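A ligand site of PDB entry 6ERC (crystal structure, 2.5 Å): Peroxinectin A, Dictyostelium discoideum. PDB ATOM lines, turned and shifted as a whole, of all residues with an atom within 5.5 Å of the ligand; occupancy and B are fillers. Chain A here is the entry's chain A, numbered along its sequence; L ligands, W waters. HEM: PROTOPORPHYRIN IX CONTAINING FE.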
ATOM      1  N   PHE A  26      13.882  -1.862 -28.845  1.00  0.00           N
ATOM      2  CA  PHE A  26      13.828  -2.106 -27.416  1.00  0.00           C
ATOM      3  C   PHE A  26      15.236  -2.218 -26.836  1.00  0.00           C
ATOM      4  O   PHE A  26      16.230  -2.380 -27.554  1.00  0.00           O
ATOM      5  CB  PHE A  26      13.051  -3.386 -27.089  1.00  0.00           C
ATOM      6  CG  PHE A  26      11.562  -3.243 -27.200  1.00  0.00           C
ATOM      7  CD1 PHE A  26      10.832  -2.627 -26.197  1.00  0.00           C
ATOM      8  CD2 PHE A  26      10.881  -3.757 -28.290  1.00  0.00           C
ATOM      9  CE1 PHE A  26       9.455  -2.501 -26.290  1.00  0.00           C
ATOM     10  CE2 PHE A  26       9.507  -3.641 -28.386  1.00  0.00           C
ATOM     11  CZ  PHE A  26       8.796  -3.017 -27.387  1.00  0.00           C
ATOM     12  N   ASN A  73      -5.353  -4.384 -11.824  1.00  0.00           N
ATOM     13  CA  ASN A  73      -4.835  -4.829 -13.113  1.00  0.00           C
ATOM     14  C   ASN A  73      -5.392  -4.008 -14.262  1.00  0.00           C
ATOM     15  O   ASN A  73      -4.769  -3.976 -15.330  1.00  0.00           O
ATOM     16  CB  ASN A  73      -5.124  -6.329 -13.316  1.00  0.00           C
ATOM     17  CG  ASN A  73      -6.542  -6.619 -13.758  1.00  0.00           C
ATOM     18  OD1 ASN A  73      -6.949  -6.273 -14.868  1.00  0.00           O
ATOM     19  ND2 ASN A  73      -7.296  -7.302 -12.900  1.00  0.00           N
ATOM     20  N   MET A  74      -6.520  -3.336 -14.066  1.00  0.00           N
ATOM     21  CA  MET A  74      -6.977  -2.370 -15.072  1.00  0.00           C
ATOM     22  C   MET A  74      -6.007  -1.216 -15.198  1.00  0.00           C
ATOM     23  O   MET A  74      -5.766  -0.715 -16.308  1.00  0.00           O
ATOM     24  CB  MET A  74      -8.378  -1.875 -14.708  1.00  0.00           C
ATOM     25  CG  MET A  74      -9.470  -2.899 -14.931  1.00  0.00           C
ATOM     26  SD  MET A  74      -9.634  -3.393 -16.659  1.00  0.00           S
ATOM     27  CE  MET A  74     -10.971  -4.579 -16.541  1.00  0.00           C
ATOM     28  N   GLY A  76      -2.745  -1.514 -14.412  1.00  0.00           N
ATOM     29  CA  GLY A  76      -1.576  -2.137 -15.014  1.00  0.00           C
ATOM     30  C   GLY A  76      -1.682  -2.204 -16.523  1.00  0.00           C
ATOM     31  O   GLY A  76      -0.747  -1.844 -17.240  1.00  0.00           O
ATOM     32  N   GLN A  77      -2.823  -2.663 -17.026  1.00  0.00           N
ATOM     33  CA  GLN A  77      -3.037  -2.697 -18.467  1.00  0.00           C
ATOM     34  C   GLN A  77      -3.055  -1.288 -19.043  1.00  0.00           C
ATOM     35  O   GLN A  77      -2.536  -1.048 -20.141  1.00  0.00           O
ATOM     36  CB  GLN A  77      -4.337  -3.437 -18.785  1.00  0.00           C
ATOM     37  CG  GLN A  77      -4.550  -3.688 -20.271  1.00  0.00           C
ATOM     38  CD  GLN A  77      -5.866  -4.390 -20.548  1.00  0.00           C
ATOM     39  OE1 GLN A  77      -6.631  -4.680 -19.623  1.00  0.00           O
ATOM     40  NE2 GLN A  77      -6.131  -4.675 -21.812  1.00  0.00           N
ATOM     41  N   ILE A  80       0.768  -0.085 -19.156  1.00  0.00           N
ATOM     42  CA  ILE A  80       1.626  -0.597 -20.229  1.00  0.00           C
ATOM     43  C   ILE A  80       1.268   0.062 -21.551  1.00  0.00           C
ATOM     44  O   ILE A  80       2.145   0.289 -22.401  1.00  0.00           O
ATOM     45  CB  ILE A  80       1.543  -2.132 -20.331  1.00  0.00           C
ATOM     46  CG1 ILE A  80       2.557  -2.642 -21.356  1.00  0.00           C
ATOM     47  CG2 ILE A  80       0.143  -2.583 -20.701  1.00  0.00           C
ATOM     48  CD1 ILE A  80       3.997  -2.532 -20.898  1.00  0.00           C
ATOM     49  N   ALA A  84       4.632   0.636 -24.105  1.00  0.00           N
ATOM     50  CA  ALA A  84       5.176  -0.315 -25.068  1.00  0.00           C
ATOM     51  C   ALA A  84       4.090  -0.886 -25.967  1.00  0.00           C
ATOM     52  O   ALA A  84       2.967  -1.145 -25.519  1.00  0.00           O
ATOM     53  CB  ALA A  84       5.885  -1.468 -24.338  1.00  0.00           C
ATOM     54  N   LEU A  85       4.439  -1.093 -27.231  1.00  0.00           N
ATOM     55  CA  LEU A  85       3.592  -1.817 -28.178  1.00  0.00           C
ATOM     56  C   LEU A  85       4.491  -2.629 -29.097  1.00  0.00           C
ATOM     57  O   LEU A  85       5.348  -2.065 -29.788  1.00  0.00           O
ATOM     58  CB  LEU A  85       2.716  -0.878 -28.996  1.00  0.00           C
ATOM     59  CG  LEU A  85       1.862  -1.578 -30.064  1.00  0.00           C
ATOM     60  CD1 LEU A  85       0.753  -2.388 -29.407  1.00  0.00           C
ATOM     61  CD2 LEU A  85       1.285  -0.583 -31.052  1.00  0.00           C
ATOM     62  N   SER A  86       4.299  -3.952 -29.110  1.00  0.00           N
ATOM     63  CA  SER A  86       5.049  -4.837 -29.991  1.00  0.00           C
ATOM     64  C   SER A  86       4.222  -5.051 -31.256  1.00  0.00           C
ATOM     65  O   SER A  86       3.579  -6.094 -31.449  1.00  0.00           O
ATOM     66  CB  SER A  86       5.379  -6.140 -29.289  1.00  0.00           C
ATOM     67  OG  SER A  86       6.199  -5.910 -28.157  1.00  0.00           O
ATOM     68  N   TYR A 116      -0.557 -15.948 -35.867  1.00  0.00           N
ATOM     69  CA  TYR A 116       0.455 -15.194 -35.135  1.00  0.00           C
ATOM     70  C   TYR A 116       1.402 -14.553 -36.129  1.00  0.00           C
ATOM     71  O   TYR A 116       1.866 -15.213 -37.068  1.00  0.00           O
ATOM     72  CB  TYR A 116       1.240 -16.081 -34.157  1.00  0.00           C
ATOM     73  CG  TYR A 116       2.337 -15.326 -33.440  1.00  0.00           C
ATOM     74  CD1 TYR A 116       3.588 -15.180 -34.003  1.00  0.00           C
ATOM     75  CD2 TYR A 116       2.115 -14.780 -32.178  1.00  0.00           C
ATOM     76  CE1 TYR A 116       4.597 -14.496 -33.352  1.00  0.00           C
ATOM     77  CE2 TYR A 116       3.115 -14.092 -31.513  1.00  0.00           C
ATOM     78  CZ  TYR A 116       4.355 -13.965 -32.106  1.00  0.00           C
ATOM     79  OH  TYR A 116       5.355 -13.285 -31.452  1.00  0.00           O
ATOM     80  N   ARG A 213      -5.593   0.065 -28.958  1.00  0.00           N
ATOM     81  CA  ARG A 213      -6.264  -1.013 -28.242  1.00  0.00           C
ATOM     82  C   ARG A 213      -6.949  -0.526 -26.972  1.00  0.00           C
ATOM     83  O   ARG A 213      -6.958  -1.209 -25.941  1.00  0.00           O
ATOM     84  CB  ARG A 213      -5.257  -2.122 -27.923  1.00  0.00           C
ATOM     85  CG  ARG A 213      -3.999  -1.655 -27.213  1.00  0.00           C
ATOM     86  CD  ARG A 213      -2.939  -2.731 -27.106  1.00  0.00           C
ATOM     87  NE  ARG A 213      -1.651  -2.146 -26.739  1.00  0.00           N
ATOM     88  CZ  ARG A 213      -0.564  -2.840 -26.399  1.00  0.00           C
ATOM     89  NH1 ARG A 213      -0.594  -4.171 -26.358  1.00  0.00           N
ATOM     90  NH2 ARG A 213       0.554  -2.197 -26.079  1.00  0.00           N
ATOM     91  N   GLU A 216     -10.084  -2.650 -25.834  1.00  0.00           N
ATOM     92  CA  GLU A 216      -9.854  -4.049 -25.501  1.00  0.00           C
ATOM     93  C   GLU A 216     -10.877  -4.548 -24.488  1.00  0.00           C
ATOM     94  O   GLU A 216     -11.471  -5.620 -24.668  1.00  0.00           O
ATOM     95  CB  GLU A 216      -8.428  -4.232 -24.965  1.00  0.00           C
ATOM     96  CG  GLU A 216      -7.904  -5.678 -25.031  1.00  0.00           C
ATOM     97  CD  GLU A 216      -8.243  -6.512 -23.800  1.00  0.00           C
ATOM     98  OE1 GLU A 216      -8.997  -6.027 -22.930  1.00  0.00           O
ATOM     99  OE2 GLU A 216      -7.745  -7.657 -23.699  1.00  0.00           O
ATOM    100  N   ASN A 217     -11.095  -3.800 -23.405  1.00  0.00           N
ATOM    101  CA  ASN A 217     -12.118  -4.168 -22.442  1.00  0.00           C
ATOM    102  C   ASN A 217     -12.725  -2.905 -21.867  1.00  0.00           C
ATOM    103  O   ASN A 217     -12.109  -1.833 -21.904  1.00  0.00           O
ATOM    104  CB  ASN A 217     -11.553  -5.055 -21.324  1.00  0.00           C
ATOM    105  CG  ASN A 217     -10.570  -4.324 -20.438  1.00  0.00           C
ATOM    106  OD1 ASN A 217     -10.977  -3.672 -19.466  1.00  0.00           O
ATOM    107  ND2 ASN A 217      -9.292  -4.430 -20.743  1.00  0.00           N
ATOM    108  N   TYR A 270       0.478   2.379  -7.461  1.00  0.00           N
ATOM    109  CA  TYR A 270       0.568   1.117  -8.183  1.00  0.00           C
ATOM    110  C   TYR A 270       1.828   0.346  -7.809  1.00  0.00           C
ATOM    111  O   TYR A 270       1.772  -0.817  -7.384  1.00  0.00           O
ATOM    112  CB  TYR A 270       0.502   1.357  -9.692  1.00  0.00           C
ATOM    113  CG  TYR A 270       0.522   0.077 -10.500  1.00  0.00           C
ATOM    114  CD1 TYR A 270      -0.627  -0.674 -10.676  1.00  0.00           C
ATOM    115  CD2 TYR A 270       1.698  -0.371 -11.096  1.00  0.00           C
ATOM    116  CE1 TYR A 270      -0.614  -1.841 -11.417  1.00  0.00           C
ATOM    117  CE2 TYR A 270       1.714  -1.540 -11.827  1.00  0.00           C
ATOM    118  CZ  TYR A 270       0.558  -2.263 -11.987  1.00  0.00           C
ATOM    119  OH  TYR A 270       0.574  -3.431 -12.719  1.00  0.00           O
ATOM    120  N   PHE A 296      11.081  -6.578 -20.086  1.00  0.00           N
ATOM    121  CA  PHE A 296      10.012  -5.972 -19.296  1.00  0.00           C
ATOM    122  C   PHE A 296       8.656  -6.202 -19.961  1.00  0.00           C
ATOM    123  O   PHE A 296       7.747  -6.776 -19.359  1.00  0.00           O
ATOM    124  CB  PHE A 296      10.287  -4.481 -19.121  1.00  0.00           C
ATOM    125  CG  PHE A 296       9.167  -3.725 -18.457  1.00  0.00           C
ATOM    126  CD1 PHE A 296       9.053  -3.687 -17.073  1.00  0.00           C
ATOM    127  CD2 PHE A 296       8.224  -3.041 -19.210  1.00  0.00           C
ATOM    128  CE1 PHE A 296       8.023  -2.987 -16.453  1.00  0.00           C
ATOM    129  CE2 PHE A 296       7.191  -2.339 -18.599  1.00  0.00           C
ATOM    130  CZ  PHE A 296       7.093  -2.316 -17.221  1.00  0.00           C
ATOM    131  N   THR A 297       8.514  -5.744 -21.202  1.00  0.00           N
ATOM    132  CA  THR A 297       7.221  -5.831 -21.870  1.00  0.00           C
ATOM    133  C   THR A 297       6.913  -7.245 -22.352  1.00  0.00           C
ATOM    134  O   THR A 297       5.746  -7.658 -22.317  1.00  0.00           O
ATOM    135  CB  THR A 297       7.170  -4.847 -23.039  1.00  0.00           C
ATOM    136  OG1 THR A 297       5.844  -4.793 -23.566  1.00  0.00           O
ATOM    137  CG2 THR A 297       8.136  -5.246 -24.153  1.00  0.00           C
ATOM    138  N   THR A 298       7.925  -7.996 -22.773  1.00  0.00           N
ATOM    139  CA  THR A 298       7.682  -9.331 -23.308  1.00  0.00           C
ATOM    140  C   THR A 298       7.459 -10.366 -22.208  1.00  0.00           C
ATOM    141  O   THR A 298       6.631 -11.265 -22.371  1.00  0.00           O
ATOM    142  CB  THR A 298       8.854  -9.761 -24.194  1.00  0.00           C
ATOM    143  OG1 THR A 298       9.160  -8.720 -25.139  1.00  0.00           O
ATOM    144  CG2 THR A 298       8.520 -11.038 -24.947  1.00  0.00           C
ATOM    145  N   PHE A 301       6.321  -7.959 -17.207  1.00  0.00           N
ATOM    146  CA  PHE A 301       5.083  -7.229 -16.962  1.00  0.00           C
ATOM    147  C   PHE A 301       3.852  -7.877 -17.595  1.00  0.00           C
ATOM    148  O   PHE A 301       2.753  -7.335 -17.454  1.00  0.00           O
ATOM    149  CB  PHE A 301       5.214  -5.792 -17.474  1.00  0.00           C
ATOM    150  CG  PHE A 301       4.317  -4.823 -16.770  1.00  0.00           C
ATOM    151  CD1 PHE A 301       4.629  -4.373 -15.491  1.00  0.00           C
ATOM    152  CD2 PHE A 301       3.154  -4.371 -17.366  1.00  0.00           C
ATOM    153  CE1 PHE A 301       3.808  -3.486 -14.840  1.00  0.00           C
ATOM    154  CE2 PHE A 301       2.321  -3.478 -16.711  1.00  0.00           C
ATOM    155  CZ  PHE A 301       2.654  -3.038 -15.450  1.00  0.00           C
ATOM    156  N   ARG A 302       4.007  -9.005 -18.280  1.00  0.00           N
ATOM    157  CA  ARG A 302       2.846  -9.734 -18.775  1.00  0.00           C
ATOM    158  C   ARG A 302       2.199 -10.598 -17.707  1.00  0.00           C
ATOM    159  O   ARG A 302       1.255 -11.333 -18.016  1.00  0.00           O
ATOM    160  CB  ARG A 302       3.238 -10.600 -19.977  1.00  0.00           C
ATOM    161  CG  ARG A 302       3.707  -9.793 -21.176  1.00  0.00           C
ATOM    162  CD  ARG A 302       3.290 -10.413 -22.494  1.00  0.00           C
ATOM    163  NE  ARG A 302       3.774  -9.625 -23.626  1.00  0.00           N
ATOM    164  CZ  ARG A 302       3.460  -9.873 -24.892  1.00  0.00           C
ATOM    165  NH1 ARG A 302       2.659 -10.880 -25.212  1.00  0.00           N
ATOM    166  NH2 ARG A 302       3.951  -9.100 -25.849  1.00  0.00           N
ATOM    167  N   PHE A 303       2.662 -10.509 -16.461  1.00  0.00           N
ATOM    168  CA  PHE A 303       2.035 -11.243 -15.364  1.00  0.00           C
ATOM    169  C   PHE A 303       0.553 -10.934 -15.227  1.00  0.00           C
ATOM    170  O   PHE A 303      -0.190 -11.736 -14.649  1.00  0.00           O
ATOM    171  CB  PHE A 303       2.753 -10.925 -14.055  1.00  0.00           C
ATOM    172  CG  PHE A 303       2.510  -9.530 -13.544  1.00  0.00           C
ATOM    173  CD1 PHE A 303       1.424  -9.248 -12.732  1.00  0.00           C
ATOM    174  CD2 PHE A 303       3.363  -8.492 -13.878  1.00  0.00           C
ATOM    175  CE1 PHE A 303       1.196  -7.969 -12.260  1.00  0.00           C
ATOM    176  CE2 PHE A 303       3.138  -7.199 -13.416  1.00  0.00           C
ATOM    177  CZ  PHE A 303       2.053  -6.949 -12.608  1.00  0.00           C
ATOM    178  N   GLY A 304       0.103  -9.773 -15.720  1.00  0.00           N
ATOM    179  CA  GLY A 304      -1.275  -9.369 -15.500  1.00  0.00           C
ATOM    180  C   GLY A 304      -2.281 -10.324 -16.098  1.00  0.00           C
ATOM    181  O   GLY A 304      -3.418 -10.407 -15.636  1.00  0.00           O
ATOM    182  N   HIS A 305      -1.889 -11.063 -17.138  1.00  0.00           N
ATOM    183  CA  HIS A 305      -2.820 -12.012 -17.738  1.00  0.00           C
ATOM    184  C   HIS A 305      -3.187 -13.125 -16.761  1.00  0.00           C
ATOM    185  O   HIS A 305      -4.291 -13.676 -16.833  1.00  0.00           O
ATOM    186  CB  HIS A 305      -2.208 -12.567 -19.014  1.00  0.00           C
ATOM    187  CG  HIS A 305      -1.809 -11.498 -19.984  1.00  0.00           C
ATOM    188  ND1 HIS A 305      -0.590 -11.487 -20.626  1.00  0.00           N
ATOM    189  CD2 HIS A 305      -2.465 -10.393 -20.410  1.00  0.00           C
ATOM    190  CE1 HIS A 305      -0.504 -10.430 -21.408  1.00  0.00           C
ATOM    191  NE2 HIS A 305      -1.637  -9.751 -21.305  1.00  0.00           N
ATOM    192  N   GLU A 307      -3.572 -12.538 -13.564  1.00  0.00           N
ATOM    193  CA  GLU A 307      -4.374 -11.927 -12.508  1.00  0.00           C
ATOM    194  C   GLU A 307      -5.760 -11.475 -12.973  1.00  0.00           C
ATOM    195  O   GLU A 307      -6.583 -11.107 -12.126  1.00  0.00           O
ATOM    196  CB  GLU A 307      -3.622 -10.730 -11.900  1.00  0.00           C
ATOM    197  CG  GLU A 307      -3.758  -9.420 -12.661  1.00  0.00           C
ATOM    198  CD  GLU A 307      -2.758  -8.367 -12.229  1.00  0.00           C
ATOM    199  OE1 GLU A 307      -2.414  -8.312 -11.024  1.00  0.00           O
ATOM    200  OE2 GLU A 307      -2.305  -7.582 -13.100  1.00  0.00           O
ATOM    201  N   VAL A 308      -6.039 -11.506 -14.279  1.00  0.00           N
ATOM    202  CA  VAL A 308      -7.365 -11.135 -14.771  1.00  0.00           C
ATOM    203  C   VAL A 308      -8.370 -12.196 -14.330  1.00  0.00           C
ATOM    204  O   VAL A 308      -8.220 -13.375 -14.642  1.00  0.00           O
ATOM    205  CB  VAL A 308      -7.337 -10.998 -16.298  1.00  0.00           C
ATOM    206  CG1 VAL A 308      -8.750 -10.837 -16.861  1.00  0.00           C
ATOM    207  CG2 VAL A 308      -6.468  -9.830 -16.707  1.00  0.00           C
ATOM    208  N   ILE A 327     -15.668 -11.968 -19.058  1.00  0.00           N
ATOM    209  CA  ILE A 327     -14.606 -11.334 -19.836  1.00  0.00           C
ATOM    210  C   ILE A 327     -14.788 -11.629 -21.316  1.00  0.00           C
ATOM    211  O   ILE A 327     -14.701 -10.729 -22.168  1.00  0.00           O
ATOM    212  CB  ILE A 327     -13.230 -11.820 -19.330  1.00  0.00           C
ATOM    213  CG1 ILE A 327     -12.927 -11.233 -17.949  1.00  0.00           C
ATOM    214  CG2 ILE A 327     -12.121 -11.459 -20.320  1.00  0.00           C
ATOM    215  CD1 ILE A 327     -12.691  -9.721 -17.939  1.00  0.00           C
ATOM    216  N   TYR A 331     -14.775  -8.366 -24.881  1.00  0.00           N
ATOM    217  CA  TYR A 331     -13.677  -8.006 -25.784  1.00  0.00           C
ATOM    218  C   TYR A 331     -14.197  -7.068 -26.858  1.00  0.00           C
ATOM    219  O   TYR A 331     -15.026  -7.464 -27.690  1.00  0.00           O
ATOM    220  CB  TYR A 331     -13.074  -9.260 -26.399  1.00  0.00           C
ATOM    221  CG  TYR A 331     -12.381 -10.191 -25.419  1.00  0.00           C
ATOM    222  CD1 TYR A 331     -11.694  -9.687 -24.321  1.00  0.00           C
ATOM    223  CD2 TYR A 331     -12.418 -11.563 -25.600  1.00  0.00           C
ATOM    224  CE1 TYR A 331     -11.059 -10.533 -23.430  1.00  0.00           C
ATOM    225  CE2 TYR A 331     -11.789 -12.422 -24.708  1.00  0.00           C
ATOM    226  CZ  TYR A 331     -11.114 -11.897 -23.626  1.00  0.00           C
ATOM    227  OH  TYR A 331     -10.489 -12.747 -22.732  1.00  0.00           O
ATOM    228  N   LEU A 364      -9.300 -16.030 -21.435  1.00  0.00           N
ATOM    229  CA  LEU A 364      -8.120 -15.570 -22.163  1.00  0.00           C
ATOM    230  C   LEU A 364      -7.398 -16.710 -22.864  1.00  0.00           C
ATOM    231  O   LEU A 364      -6.901 -16.538 -23.984  1.00  0.00           O
ATOM    232  CB  LEU A 364      -7.159 -14.874 -21.201  1.00  0.00           C
ATOM    233  CG  LEU A 364      -7.671 -13.618 -20.488  1.00  0.00           C
ATOM    234  CD1 LEU A 364      -6.866 -13.356 -19.232  1.00  0.00           C
ATOM    235  CD2 LEU A 364      -7.608 -12.408 -21.414  1.00  0.00           C
ATOM    236  N   LEU A 379      -4.185 -16.437 -25.280  1.00  0.00           N
ATOM    237  CA  LEU A 379      -3.254 -15.399 -24.839  1.00  0.00           C
ATOM    238  C   LEU A 379      -2.013 -15.985 -24.197  1.00  0.00           C
ATOM    239  O   LEU A 379      -0.921 -15.434 -24.342  1.00  0.00           O
ATOM    240  CB  LEU A 379      -3.970 -14.442 -23.886  1.00  0.00           C
ATOM    241  CG  LEU A 379      -3.195 -13.197 -23.459  1.00  0.00           C
ATOM    242  CD1 LEU A 379      -2.610 -12.447 -24.647  1.00  0.00           C
ATOM    243  CD2 LEU A 379      -4.119 -12.276 -22.679  1.00  0.00           C
ATOM    244  N   ARG A 382       0.079 -16.947 -27.154  1.00  0.00           N
ATOM    245  CA  ARG A 382       0.629 -15.759 -27.779  1.00  0.00           C
ATOM    246  C   ARG A 382       1.833 -15.228 -27.004  1.00  0.00           C
ATOM    247  O   ARG A 382       2.814 -14.770 -27.598  1.00  0.00           O
ATOM    248  CB  ARG A 382      -0.453 -14.674 -27.910  1.00  0.00           C
ATOM    249  CG  ARG A 382      -1.504 -14.994 -28.960  1.00  0.00           C
ATOM    250  CD  ARG A 382      -2.369 -13.778 -29.290  1.00  0.00           C
ATOM    251  NE  ARG A 382      -1.663 -12.803 -30.122  1.00  0.00           N
ATOM    252  CZ  ARG A 382      -1.506 -12.904 -31.442  1.00  0.00           C
ATOM    253  NH1 ARG A 382      -2.002 -13.945 -32.099  1.00  0.00           N
ATOM    254  NH2 ARG A 382      -0.843 -11.968 -32.118  1.00  0.00           N
ATOM    255  N   ASN A 383       1.767 -15.291 -25.677  1.00  0.00           N
ATOM    256  CA  ASN A 383       2.900 -14.835 -24.868  1.00  0.00           C
ATOM    257  C   ASN A 383       4.121 -15.719 -25.083  1.00  0.00           C
ATOM    258  O   ASN A 383       5.222 -15.212 -25.309  1.00  0.00           O
ATOM    259  CB  ASN A 383       2.504 -14.788 -23.397  1.00  0.00           C
ATOM    260  CG  ASN A 383       1.391 -13.803 -23.120  1.00  0.00           C
ATOM    261  OD1 ASN A 383       1.293 -12.755 -23.763  1.00  0.00           O
ATOM    262  ND2 ASN A 383       0.527 -14.126 -22.158  1.00  0.00           N
ATOM    263  N   ARG A 386       5.609 -14.922 -28.347  1.00  0.00           N
ATOM    264  CA  ARG A 386       6.275 -13.632 -28.355  1.00  0.00           C
ATOM    265  C   ARG A 386       7.642 -13.716 -27.675  1.00  0.00           C
ATOM    266  O   ARG A 386       8.621 -13.131 -28.160  1.00  0.00           O
ATOM    267  CB  ARG A 386       5.395 -12.578 -27.667  1.00  0.00           C
ATOM    268  CG  ARG A 386       5.811 -11.129 -27.918  1.00  0.00           C
ATOM    269  CD  ARG A 386       5.531 -10.691 -29.340  1.00  0.00           C
ATOM    270  NE  ARG A 386       4.130 -10.879 -29.724  1.00  0.00           N
ATOM    271  CZ  ARG A 386       3.650 -10.666 -30.942  1.00  0.00           C
ATOM    272  NH1 ARG A 386       4.455 -10.264 -31.920  1.00  0.00           N
ATOM    273  NH2 ARG A 386       2.365 -10.871 -31.205  1.00  0.00           N
HETATM  274  CHA HEM L   1       0.064  -7.637 -24.395  1.00  0.00           C
HETATM  275  CHB HEM L   1      -4.646  -8.681 -23.974  1.00  0.00           C
HETATM  276  CHC HEM L   1      -4.479  -7.422 -19.284  1.00  0.00           C
HETATM  277  CHD HEM L   1       0.285  -6.617 -19.663  1.00  0.00           C
HETATM  278  C1A HEM L   1      -1.211  -8.087 -24.667  1.00  0.00           C
HETATM  279  C2A HEM L   1      -1.643  -8.699 -25.895  1.00  0.00           C
HETATM  280  C3A HEM L   1      -2.943  -8.989 -25.795  1.00  0.00           C
HETATM  281  C4A HEM L   1      -3.380  -8.564 -24.481  1.00  0.00           C
HETATM  282  CMA HEM L   1      -3.840  -9.662 -26.858  1.00  0.00           C
HETATM  283  CAA HEM L   1      -0.723  -8.963 -27.107  1.00  0.00           C
HETATM  284  CBA HEM L   1      -0.579 -10.482 -27.212  1.00  0.00           C
HETATM  285  CGA HEM L   1       0.694 -10.822 -27.950  1.00  0.00           C
HETATM  286  O1A HEM L   1       1.799 -10.485 -27.440  1.00  0.00           O
HETATM  287  O2A HEM L   1       0.607 -11.428 -29.041  1.00  0.00           O
HETATM  288  C1B HEM L   1      -5.003  -8.408 -22.680  1.00  0.00           C
HETATM  289  C2B HEM L   1      -6.339  -8.525 -22.140  1.00  0.00           C
HETATM  290  C3B HEM L   1      -6.306  -8.176 -20.851  1.00  0.00           C
HETATM  291  C4B HEM L   1      -4.930  -7.824 -20.515  1.00  0.00           C
HETATM  292  CMB HEM L   1      -7.532  -8.978 -23.005  1.00  0.00           C
HETATM  293  CAB HEM L   1      -7.447  -8.127 -19.806  1.00  0.00           C
HETATM  294  CBB HEM L   1      -8.696  -8.526 -20.070  1.00  0.00           C
HETATM  295  C1C HEM L   1      -3.180  -7.105 -18.960  1.00  0.00           C
HETATM  296  C2C HEM L   1      -2.681  -6.691 -17.658  1.00  0.00           C
HETATM  297  C3C HEM L   1      -1.358  -6.465 -17.772  1.00  0.00           C
HETATM  298  C4C HEM L   1      -0.991  -6.730 -19.142  1.00  0.00           C
HETATM  299  CMC HEM L   1      -3.612  -6.576 -16.428  1.00  0.00           C
HETATM  300  CAC HEM L   1      -0.279  -6.012 -16.746  1.00  0.00           C
HETATM  301  CBC HEM L   1      -0.489  -5.726 -15.464  1.00  0.00           C
HETATM  302  C1D HEM L   1       0.622  -6.773 -20.980  1.00  0.00           C
HETATM  303  C2D HEM L   1       1.918  -6.509 -21.565  1.00  0.00           C
HETATM  304  C3D HEM L   1       1.851  -6.804 -22.859  1.00  0.00           C
HETATM  305  C4D HEM L   1       0.510  -7.248 -23.163  1.00  0.00           C
HETATM  306  CMD HEM L   1       3.147  -6.004 -20.779  1.00  0.00           C
HETATM  307  CAD HEM L   1       2.966  -6.664 -23.917  1.00  0.00           C
HETATM  308  CBD HEM L   1       2.994  -5.185 -24.289  1.00  0.00           C
HETATM  309  CGD HEM L   1       3.351  -4.991 -25.742  1.00  0.00           C
HETATM  310  O1D HEM L   1       2.425  -5.060 -26.593  1.00  0.00           O
HETATM  311  O2D HEM L   1       4.541  -4.758 -26.057  1.00  0.00           O
HETATM  312  NA  HEM L   1      -2.292  -8.015 -23.827  1.00  0.00           N
HETATM  313  NB  HEM L   1      -4.175  -7.976 -21.665  1.00  0.00           N
HETATM  314  NC  HEM L   1      -2.116  -7.109 -19.840  1.00  0.00           N
HETATM  315  ND  HEM L   1      -0.207  -7.229 -21.988  1.00  0.00           N
HETATM  316 FE   HEM L   1      -2.174  -7.540 -21.835  1.00  0.00          FE
HETATM  317  O   HOH W   1      -2.612  -5.425 -23.855  1.00  0.00           O
HETATM  318  O   HOH W   2      -1.526  -4.845 -12.300  1.00  0.00           O
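An oxygen (O2D) of the ligand sits at hydrogen-bond distance from the side-chain hydroxyl (OG1) of Thr 297 (2.8 Å). An iron atom (FE) of the ligand is bound by a ring nitrogen (NE2) of His 305 (2.3 Å). NH2 of Arg 386 is in salt-bridge range of O2A of the ligand, at 2.8 Å. OE2 of Glu 216 is bonded to CMB of the ligand (1.5 Å). The side-chain hydroxyl of Ser 86 lies within hydrogen-bond range of an oxygen (O2D) of the ligand (2.9 Å). N of Ser 86 sits at hydrogen-bond distance from O2D of the ligand (3.2 Å). NH1 of Arg 213 is in salt-bridge range of O1D of the ligand, at 3.2 Å. NH1 of Arg 302 is in salt-bridge range of O1A of the ligand (2.4 Å). The guanidinium group (NE) of Arg 382 is in salt-bridge range of an oxygen (O2A) of the ligand (2.9 Å).
NH1 of Arg 302 lies within hydrogen-bond range of OD1 of Asn 383. The backbone carbonyl oxygen (O) of Ala 84 lies within hydrogen-bond range of the guanidinium group (NH2) of Arg 213 (2.7 Å). The backbone carbonyl oxygen of Leu 379 is in hydrogen-bond range of the side-chain amide nitrogen of Asn 383, 2.9 Å away. The backbone carbonyl oxygen (O) of Arg 302 is in hydrogen-bond range of a ring nitrogen (ND1) of His 305. ND1 of His 305 sits at hydrogen-bond distance from ND2 of Asn 383 (3.2 Å). The side-chain carboxylate (OE1) of Glu 216 sits at hydrogen-bond distance from the side-chain amide nitrogen (ND2) of Asn 217, at 2.7 Å. The guanidinium group (NH1) of Arg 386 lies close to the side-chain hydroxyl (OH) of Tyr 116 (3.2 Å). OE1 of Glu 216 lies within hydrogen-bond range of NE2 of Gln 77 (3.4 Å).
Water W2 bridges OH of Tyr 270 (2.6 Å) and OE2 of Glu 307 (3.0 Å).
O of Asn 73 touches CMC of the ligand, 3.1 Å away. Gly 76 touches the ligand (CA to CBC, 3.8 Å). Gln 77 touches the ligand (OE1 to CHC, 3.5 Å). CG1 of Ile 80 touches CMD of the ligand, 3.5 Å away. Ala 84 touches the ligand. C of Leu 85 touches O2D of the ligand, 3.7 Å away. Tyr 270 touches the ligand (OH to CBC, 3.7 Å). Phe 301 touches the ligand (O to CAC, 3.4 Å). CA of Gly 304 touches C3C of the ligand, 3.7 Å away. OE2 of Glu 307 touches CBC of the ligand (3.5 Å). Val 308 touches the ligand (CG2 to CAB, 3.7 Å). CE1 of Tyr 331 touches CMB of the ligand, at 3.9 Å. Leu 364 touches the ligand. Leu 379 touches the ligand. Hydrophobic or aromatic side chains within 4 Å of the ligand: Ile 80, Ala 84, Phe 301, His 305, Val 308, Tyr 331, Leu 364 and Leu 379. The nearest printed residue that does not touch the ligand is Phe 303 (4.01 Å).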
